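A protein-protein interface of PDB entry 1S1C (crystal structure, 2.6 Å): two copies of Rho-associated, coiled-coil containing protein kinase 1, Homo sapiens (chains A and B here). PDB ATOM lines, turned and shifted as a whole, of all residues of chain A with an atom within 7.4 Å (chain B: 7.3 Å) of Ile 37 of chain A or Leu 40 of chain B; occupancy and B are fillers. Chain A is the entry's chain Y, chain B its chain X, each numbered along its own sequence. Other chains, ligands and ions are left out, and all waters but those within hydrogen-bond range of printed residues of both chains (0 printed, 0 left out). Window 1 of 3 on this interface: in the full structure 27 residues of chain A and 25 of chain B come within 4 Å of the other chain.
Ile 37 of chain A touches Glu 36 of chain B, but with the chains exchanged Glu 36 of chain A does not touch Ile 37 of chain B (4.5 Å).
Ile 37 of chain A touches Leu 40 of chain B, but with the chains exchanged Leu 40 of chain A does not touch Ile 37 of chain B (4.8 Å).
Leu 40 of chain A touches Lys 41 of chain B, but with the chains exchanged Lys 41 of chain A does not touch Leu 40 of chain B (4.3 Å).
Lys 41 of chain A touches Phe 44 of chain B, and with the chains exchanged Phe 44 of chain A touches Lys 41 of chain B.
Of the 10 pairs that touch across the chains among the printed residues, 6 have their exchanged pair printed and touching as well.
The side-chain carboxylate of Glu 32 of chain A is in salt-bridge range of the side-chain amino group of Lys 33 of chain B.
NZ of Lys 33 of chain B lies within salt-bridge range of OE2 of Glu 36 of chain A, 3.1 Å away.
NZ of Lys 33 of chain A lies within salt-bridge range of OE1 of Glu 36 of chain B (2.7 Å).
Among the printed residues, 10 pairs touch across the chains.
Among the printed residues, Asp or Glu carboxylates within 4 Å of a Lys or Arg side-chain nitrogen of the other chain: Glu 32 of chain A with Lys 33 of chain B (3.9 Å), Lys 33 of chain A with Glu 36 of chain B (2.7 Å) and Glu 36 of chain A with Lys 33 of chain B (3.1 Å).
Among the printed residues, pairs that only touch across the chains: Phe 44 of chain A with Phe 44 of chain B (3.1 Å), Ile 37 of chain A with Glu 36 of chain B (3.2 Å), Leu 40 of chain A with Leu 40 of chain B (3.6 Å), Phe 44 of chain A with Lys 41 of chain B (3.8 Å), Lys 41 of chain A with Phe 44 of chain B (3.9 Å), Leu 40 of chain A with Lys 41 of chain B (3.95 Å) and Ile 37 of chain A with Leu 40 of chain B (3.96 Å).
Printed residues of chain B within 4 Å of Glu 32 of chain A: Lys 33 (3.9 Å).
Printed residues of chain B within 4 Å of Glu 36 of chain A: Lys 33.
Of chain B, only Glu 36 (3.2 Å) and Leu 40 (3.96 Å) come within 4 Å of Ile 37 of chain A.
Of the printed residues of chain B, Phe 44 of chain A touches Lys 41 and Phe 44.
Leu 40 of chain B touches two residues of chain A.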
ATOM      1  N   GLU A  32      17.631 -13.873   4.908  1.00  0.00           N
ATOM      2  CA  GLU A  32      18.018 -12.486   4.710  1.00  0.00           C
ATOM      3  C   GLU A  32      16.808 -11.607   4.972  1.00  0.00           C
ATOM      4  O   GLU A  32      16.927 -10.478   5.445  1.00  0.00           O
ATOM      5  CB  GLU A  32      18.496 -12.299   3.281  1.00  0.00           C
ATOM      6  CG  GLU A  32      19.681 -11.392   3.167  1.00  0.00           C
ATOM      7  CD  GLU A  32      20.469 -11.672   1.920  1.00  0.00           C
ATOM      8  OE1 GLU A  32      19.904 -11.496   0.820  1.00  0.00           O
ATOM      9  OE2 GLU A  32      21.647 -12.079   2.044  1.00  0.00           O
ATOM     10  N   LYS A  33      15.643 -12.147   4.640  1.00  0.00           N
ATOM     11  CA  LYS A  33      14.366 -11.478   4.844  1.00  0.00           C
ATOM     12  C   LYS A  33      14.013 -11.649   6.329  1.00  0.00           C
ATOM     13  O   LYS A  33      13.569 -10.712   6.995  1.00  0.00           O
ATOM     14  CB  LYS A  33      13.315 -12.147   3.949  1.00  0.00           C
ATOM     15  CG  LYS A  33      11.894 -11.639   4.081  1.00  0.00           C
ATOM     16  CD  LYS A  33      10.958 -12.475   3.208  1.00  0.00           C
ATOM     17  CE  LYS A  33       9.536 -11.934   3.215  1.00  0.00           C
ATOM     18  NZ  LYS A  33       8.587 -12.760   2.407  1.00  0.00           N
ATOM     19  N   GLU A  34      14.249 -12.858   6.834  1.00  0.00           N
ATOM     20  CA  GLU A  34      13.983 -13.222   8.226  1.00  0.00           C
ATOM     21  C   GLU A  34      14.721 -12.355   9.244  1.00  0.00           C
ATOM     22  O   GLU A  34      14.263 -12.190  10.375  1.00  0.00           O
ATOM     23  CB  GLU A  34      14.353 -14.694   8.455  1.00  0.00           C
ATOM     24  CG  GLU A  34      14.134 -15.197   9.882  1.00  0.00           C
ATOM     25  CD  GLU A  34      15.404 -15.751  10.508  1.00  0.00           C
ATOM     26  OE1 GLU A  34      16.341 -14.960  10.763  1.00  0.00           O
ATOM     27  OE2 GLU A  34      15.463 -16.980  10.738  1.00  0.00           O
ATOM     28  N   GLU A  35      15.871 -11.822   8.853  1.00  0.00           N
ATOM     29  CA  GLU A  35      16.641 -10.971   9.743  1.00  0.00           C
ATOM     30  C   GLU A  35      16.274  -9.513   9.509  1.00  0.00           C
ATOM     31  O   GLU A  35      16.108  -8.746  10.456  1.00  0.00           O
ATOM     32  CB  GLU A  35      18.139 -11.164   9.507  1.00  0.00           C
ATOM     33  CG  GLU A  35      18.850 -11.906  10.623  1.00  0.00           C
ATOM     34  CD  GLU A  35      20.356 -11.907  10.453  1.00  0.00           C
ATOM     35  OE1 GLU A  35      20.977 -10.821  10.536  1.00  0.00           O
ATOM     36  OE2 GLU A  35      20.920 -12.999  10.231  1.00  0.00           O
ATOM     37  N   GLU A  36      16.142  -9.142   8.239  1.00  0.00           N
ATOM     38  CA  GLU A  36      15.808  -7.773   7.874  1.00  0.00           C
ATOM     39  C   GLU A  36      14.546  -7.328   8.595  1.00  0.00           C
ATOM     40  O   GLU A  36      14.521  -6.283   9.238  1.00  0.00           O
ATOM     41  CB  GLU A  36      15.628  -7.663   6.357  1.00  0.00           C
ATOM     42  CG  GLU A  36      15.632  -6.233   5.847  1.00  0.00           C
ATOM     43  CD  GLU A  36      16.189  -6.133   4.444  1.00  0.00           C
ATOM     44  OE1 GLU A  36      16.275  -5.004   3.911  1.00  0.00           O
ATOM     45  OE2 GLU A  36      16.545  -7.190   3.879  1.00  0.00           O
ATOM     46  N   ILE A  37      13.499  -8.134   8.490  1.00  0.00           N
ATOM     47  CA  ILE A  37      12.242  -7.824   9.152  1.00  0.00           C
ATOM     48  C   ILE A  37      12.467  -7.838  10.658  1.00  0.00           C
ATOM     49  O   ILE A  37      12.023  -6.934  11.354  1.00  0.00           O
ATOM     50  CB  ILE A  37      11.163  -8.845   8.775  1.00  0.00           C
ATOM     51  CG1 ILE A  37      10.899  -8.763   7.270  1.00  0.00           C
ATOM     52  CG2 ILE A  37       9.888  -8.573   9.549  1.00  0.00           C
ATOM     53  CD1 ILE A  37       9.927  -9.804   6.755  1.00  0.00           C
ATOM     54  N   SER A  38      13.173  -8.857  11.149  1.00  0.00           N
ATOM     55  CA  SER A  38      13.476  -8.991  12.578  1.00  0.00           C
ATOM     56  C   SER A  38      14.062  -7.725  13.177  1.00  0.00           C
ATOM     57  O   SER A  38      13.413  -7.040  13.965  1.00  0.00           O
ATOM     58  CB  SER A  38      14.467 -10.132  12.831  1.00  0.00           C
ATOM     59  OG  SER A  38      13.823 -11.390  12.815  1.00  0.00           O
ATOM     60  N   ASN A  39      15.302  -7.428  12.807  1.00  0.00           N
ATOM     61  CA  ASN A  39      15.986  -6.249  13.317  1.00  0.00           C
ATOM     62  C   ASN A  39      15.196  -4.972  13.032  1.00  0.00           C
ATOM     63  O   ASN A  39      15.283  -4.001  13.785  1.00  0.00           O
ATOM     64  CB  ASN A  39      17.391  -6.152  12.711  1.00  0.00           C
ATOM     65  CG  ASN A  39      18.264  -7.348  13.061  1.00  0.00           C
ATOM     66  OD1 ASN A  39      19.492  -7.275  12.985  1.00  0.00           O
ATOM     67  ND2 ASN A  39      17.635  -8.456  13.439  1.00  0.00           N
ATOM     68  N   LEU A  40      14.421  -4.980  11.951  1.00  0.00           N
ATOM     69  CA  LEU A  40      13.609  -3.827  11.581  1.00  0.00           C
ATOM     70  C   LEU A  40      12.489  -3.623  12.606  1.00  0.00           C
ATOM     71  O   LEU A  40      12.428  -2.591  13.273  1.00  0.00           O
ATOM     72  CB  LEU A  40      13.025  -4.038  10.182  1.00  0.00           C
ATOM     73  CG  LEU A  40      12.178  -2.923   9.571  1.00  0.00           C
ATOM     74  CD1 LEU A  40      12.092  -3.137   8.071  1.00  0.00           C
ATOM     75  CD2 LEU A  40      10.788  -2.903  10.209  1.00  0.00           C
ATOM     76  N   LYS A  41      11.608  -4.611  12.729  1.00  0.00           N
ATOM     77  CA  LYS A  41      10.508  -4.536  13.681  1.00  0.00           C
ATOM     78  C   LYS A  41      11.040  -4.333  15.091  1.00  0.00           C
ATOM     79  O   LYS A  41      10.381  -3.718  15.926  1.00  0.00           O
ATOM     80  CB  LYS A  41       9.673  -5.817  13.641  1.00  0.00           C
ATOM     81  CG  LYS A  41       8.860  -6.007  12.367  1.00  0.00           C
ATOM     82  CD  LYS A  41       8.040  -7.300  12.417  1.00  0.00           C
ATOM     83  CE  LYS A  41       7.014  -7.281  13.549  1.00  0.00           C
ATOM     84  NZ  LYS A  41       6.160  -8.500  13.539  1.00  0.00           N
ATOM     85  N   ALA A  42      12.232  -4.864  15.352  1.00  0.00           N
ATOM     86  CA  ALA A  42      12.867  -4.738  16.664  1.00  0.00           C
ATOM     87  C   ALA A  42      13.039  -3.269  17.029  1.00  0.00           C
ATOM     88  O   ALA A  42      12.595  -2.824  18.086  1.00  0.00           O
ATOM     89  CB  ALA A  42      14.224  -5.430  16.654  1.00  0.00           C
ATOM     90  N   ALA A  43      13.689  -2.524  16.139  1.00  0.00           N
ATOM     91  CA  ALA A  43      13.934  -1.100  16.331  1.00  0.00           C
ATOM     92  C   ALA A  43      12.636  -0.292  16.216  1.00  0.00           C
ATOM     93  O   ALA A  43      12.353   0.555  17.061  1.00  0.00           O
ATOM     94  CB  ALA A  43      14.956  -0.612  15.298  1.00  0.00           C
ATOM     95  N   PHE A  44      11.857  -0.561  15.167  1.00  0.00           N
ATOM     96  CA  PHE A  44      10.589   0.132  14.920  1.00  0.00           C
ATOM     97  C   PHE A  44       9.550  -0.126  16.017  1.00  0.00           C
ATOM     98  O   PHE A  44       8.394   0.284  15.894  1.00  0.00           O
ATOM     99  CB  PHE A  44      10.010  -0.296  13.564  1.00  0.00           C
ATOM    100  CG  PHE A  44      10.782   0.220  12.369  1.00  0.00           C
ATOM    101  CD1 PHE A  44      12.162   0.432  12.438  1.00  0.00           C
ATOM    102  CD2 PHE A  44      10.130   0.455  11.156  1.00  0.00           C
ATOM    103  CE1 PHE A  44      12.882   0.871  11.314  1.00  0.00           C
ATOM    104  CE2 PHE A  44      10.838   0.894  10.025  1.00  0.00           C
ATOM    105  CZ  PHE A  44      12.218   1.101  10.105  1.00  0.00           C
ATOM    106  N   LYS B  33      10.086  -9.362  -1.191  1.00  0.00           N
ATOM    107  CA  LYS B  33      10.853  -8.788  -0.089  1.00  0.00           C
ATOM    108  C   LYS B  33      10.811  -7.256  -0.124  1.00  0.00           C
ATOM    109  O   LYS B  33      10.989  -6.606   0.907  1.00  0.00           O
ATOM    110  CB  LYS B  33      12.310  -9.270  -0.172  1.00  0.00           C
ATOM    111  CG  LYS B  33      13.229  -8.827   0.969  1.00  0.00           C
ATOM    112  CD  LYS B  33      14.689  -9.024   0.577  1.00  0.00           C
ATOM    113  CE  LYS B  33      15.645  -8.732   1.717  1.00  0.00           C
ATOM    114  NZ  LYS B  33      17.063  -8.931   1.320  1.00  0.00           N
ATOM    115  N   GLU B  34      10.572  -6.680  -1.304  1.00  0.00           N
ATOM    116  CA  GLU B  34      10.523  -5.224  -1.443  1.00  0.00           C
ATOM    117  C   GLU B  34       9.172  -4.610  -1.100  1.00  0.00           C
ATOM    118  O   GLU B  34       9.108  -3.488  -0.602  1.00  0.00           O
ATOM    119  CB  GLU B  34      10.906  -4.798  -2.859  1.00  0.00           C
ATOM    120  CG  GLU B  34      11.007  -3.292  -3.004  1.00  0.00           C
ATOM    121  CD  GLU B  34      11.568  -2.856  -4.340  1.00  0.00           C
ATOM    122  OE1 GLU B  34      12.649  -3.349  -4.729  1.00  0.00           O
ATOM    123  OE2 GLU B  34      10.932  -2.009  -5.001  1.00  0.00           O
ATOM    124  N   GLU B  35       8.094  -5.334  -1.379  1.00  0.00           N
ATOM    125  CA  GLU B  35       6.758  -4.839  -1.081  1.00  0.00           C
ATOM    126  C   GLU B  35       6.470  -5.054   0.396  1.00  0.00           C
ATOM    127  O   GLU B  35       5.999  -4.150   1.082  1.00  0.00           O
ATOM    128  CB  GLU B  35       5.720  -5.571  -1.932  1.00  0.00           C
ATOM    129  N   GLU B  36       6.777  -6.253   0.884  1.00  0.00           N
ATOM    130  CA  GLU B  36       6.545  -6.598   2.280  1.00  0.00           C
ATOM    131  C   GLU B  36       7.232  -5.619   3.245  1.00  0.00           C
ATOM    132  O   GLU B  36       6.916  -5.599   4.437  1.00  0.00           O
ATOM    133  CB  GLU B  36       7.007  -8.036   2.552  1.00  0.00           C
ATOM    134  CG  GLU B  36       6.377  -8.665   3.787  1.00  0.00           C
ATOM    135  CD  GLU B  36       6.783 -10.120   3.995  1.00  0.00           C
ATOM    136  OE1 GLU B  36       6.659 -10.923   3.040  1.00  0.00           O
ATOM    137  OE2 GLU B  36       7.214 -10.458   5.123  1.00  0.00           O
ATOM    138  N   ILE B  37       8.170  -4.813   2.739  1.00  0.00           N
ATOM    139  CA  ILE B  37       8.857  -3.821   3.578  1.00  0.00           C
ATOM    140  C   ILE B  37       8.498  -2.400   3.151  1.00  0.00           C
ATOM    141  O   ILE B  37       8.506  -1.480   3.971  1.00  0.00           O
ATOM    142  CB  ILE B  37      10.418  -3.946   3.538  1.00  0.00           C
ATOM    143  CG1 ILE B  37      10.961  -3.582   2.153  1.00  0.00           C
ATOM    144  CG2 ILE B  37      10.836  -5.346   3.950  1.00  0.00           C
ATOM    145  CD1 ILE B  37      12.481  -3.472   2.100  1.00  0.00           C
ATOM    146  N   SER B  38       8.184  -2.227   1.867  1.00  0.00           N
ATOM    147  CA  SER B  38       7.826  -0.915   1.336  1.00  0.00           C
ATOM    148  C   SER B  38       6.548  -0.425   2.002  1.00  0.00           C
ATOM    149  O   SER B  38       6.115   0.709   1.782  1.00  0.00           O
ATOM    150  CB  SER B  38       7.643  -0.974  -0.189  1.00  0.00           C
ATOM    151  OG  SER B  38       6.534  -1.773  -0.571  1.00  0.00           O
ATOM    152  N   ASN B  39       5.953  -1.291   2.819  1.00  0.00           N
ATOM    153  CA  ASN B  39       4.735  -0.957   3.538  1.00  0.00           C
ATOM    154  C   ASN B  39       4.899  -1.305   5.013  1.00  0.00           C
ATOM    155  O   ASN B  39       4.110  -0.875   5.850  1.00  0.00           O
ATOM    156  CB  ASN B  39       3.527  -1.701   2.940  1.00  0.00           C
ATOM    157  CG  ASN B  39       3.198  -3.000   3.674  1.00  0.00           C
ATOM    158  OD1 ASN B  39       3.517  -4.095   3.207  1.00  0.00           O
ATOM    159  ND2 ASN B  39       2.550  -2.878   4.831  1.00  0.00           N
ATOM    160  N   LEU B  40       5.922  -2.093   5.330  1.00  0.00           N
ATOM    161  CA  LEU B  40       6.177  -2.462   6.718  1.00  0.00           C
ATOM    162  C   LEU B  40       6.798  -1.242   7.393  1.00  0.00           C
ATOM    163  O   LEU B  40       6.714  -1.080   8.611  1.00  0.00           O
ATOM    164  CB  LEU B  40       7.141  -3.650   6.803  1.00  0.00           C
ATOM    165  CG  LEU B  40       7.318  -4.311   8.180  1.00  0.00           C
ATOM    166  CD1 LEU B  40       6.177  -5.283   8.443  1.00  0.00           C
ATOM    167  CD2 LEU B  40       8.642  -5.059   8.223  1.00  0.00           C
ATOM    168  N   LYS B  41       7.428  -0.386   6.593  1.00  0.00           N
ATOM    169  CA  LYS B  41       8.044   0.824   7.109  1.00  0.00           C
ATOM    170  C   LYS B  41       6.998   1.920   7.130  1.00  0.00           C
ATOM    171  O   LYS B  41       6.708   2.495   8.180  1.00  0.00           O
ATOM    172  CB  LYS B  41       9.221   1.253   6.228  1.00  0.00           C
ATOM    173  CG  LYS B  41      10.411   0.305   6.281  1.00  0.00           C
ATOM    174  CD  LYS B  41      11.646   0.897   5.606  1.00  0.00           C
ATOM    175  CE  LYS B  41      12.866   0.003   5.800  1.00  0.00           C
ATOM    176  NZ  LYS B  41      14.110   0.615   5.256  1.00  0.00           N
ATOM    177  N   ALA B  42       6.422   2.198   5.966  1.00  0.00           N
ATOM    178  CA  ALA B  42       5.403   3.231   5.851  1.00  0.00           C
ATOM    179  C   ALA B  42       4.293   3.024   6.878  1.00  0.00           C
ATOM    180  O   ALA B  42       3.556   3.954   7.206  1.00  0.00           O
ATOM    181  CB  ALA B  42       4.826   3.239   4.446  1.00  0.00           C
ATOM    182  N   ALA B  43       4.175   1.803   7.389  1.00  0.00           N
ATOM    183  CA  ALA B  43       3.160   1.503   8.394  1.00  0.00           C
ATOM    184  C   ALA B  43       3.699   1.872   9.771  1.00  0.00           C
ATOM    185  O   ALA B  43       2.970   2.417  10.601  1.00  0.00           O
ATOM    186  CB  ALA B  43       2.788   0.025   8.354  1.00  0.00           C
ATOM    187  N   PHE B  44       4.975   1.573  10.013  1.00  0.00           N
ATOM    188  CA  PHE B  44       5.601   1.901  11.291  1.00  0.00           C
ATOM    189  C   PHE B  44       5.779   3.411  11.420  1.00  0.00           C
ATOM    190  O   PHE B  44       5.948   3.926  12.526  1.00  0.00           O
ATOM    191  CB  PHE B  44       6.965   1.213  11.440  1.00  0.00           C
ATOM    192  CG  PHE B  44       6.900  -0.149  12.081  1.00  0.00           C
ATOM    193  CD1 PHE B  44       7.108  -1.302  11.327  1.00  0.00           C
ATOM    194  CD2 PHE B  44       6.619  -0.279  13.442  1.00  0.00           C
ATOM    195  CE1 PHE B  44       7.038  -2.573  11.916  1.00  0.00           C
ATOM    196  CE2 PHE B  44       6.545  -1.544  14.043  1.00  0.00           C
ATOM    197  CZ  PHE B  44       6.755  -2.693  13.275  1.00  0.00           C
ATOM    198  N   GLU B  45       5.740   4.119  10.292  1.00  0.00           N
ATOM    199  CA  GLU B  45       5.892   5.569  10.305  1.00  0.00           C
ATOM    200  C   GLU B  45       4.619   6.268  10.748  1.00  0.00           C
ATOM    201  O   GLU B  45       4.632   7.050  11.698  1.00  0.00           O
ATOM    202  CB  GLU B  45       6.285   6.099   8.929  1.00  0.00           C
ATOM    203  CG  GLU B  45       6.372   7.621   8.908  1.00  0.00           C
ATOM    204  CD  GLU B  45       6.954   8.167   7.621  1.00  0.00           C
ATOM    205  OE1 GLU B  45       6.298   8.034   6.566  1.00  0.00           O
ATOM    206  OE2 GLU B  45       8.073   8.729   7.669  1.00  0.00           O
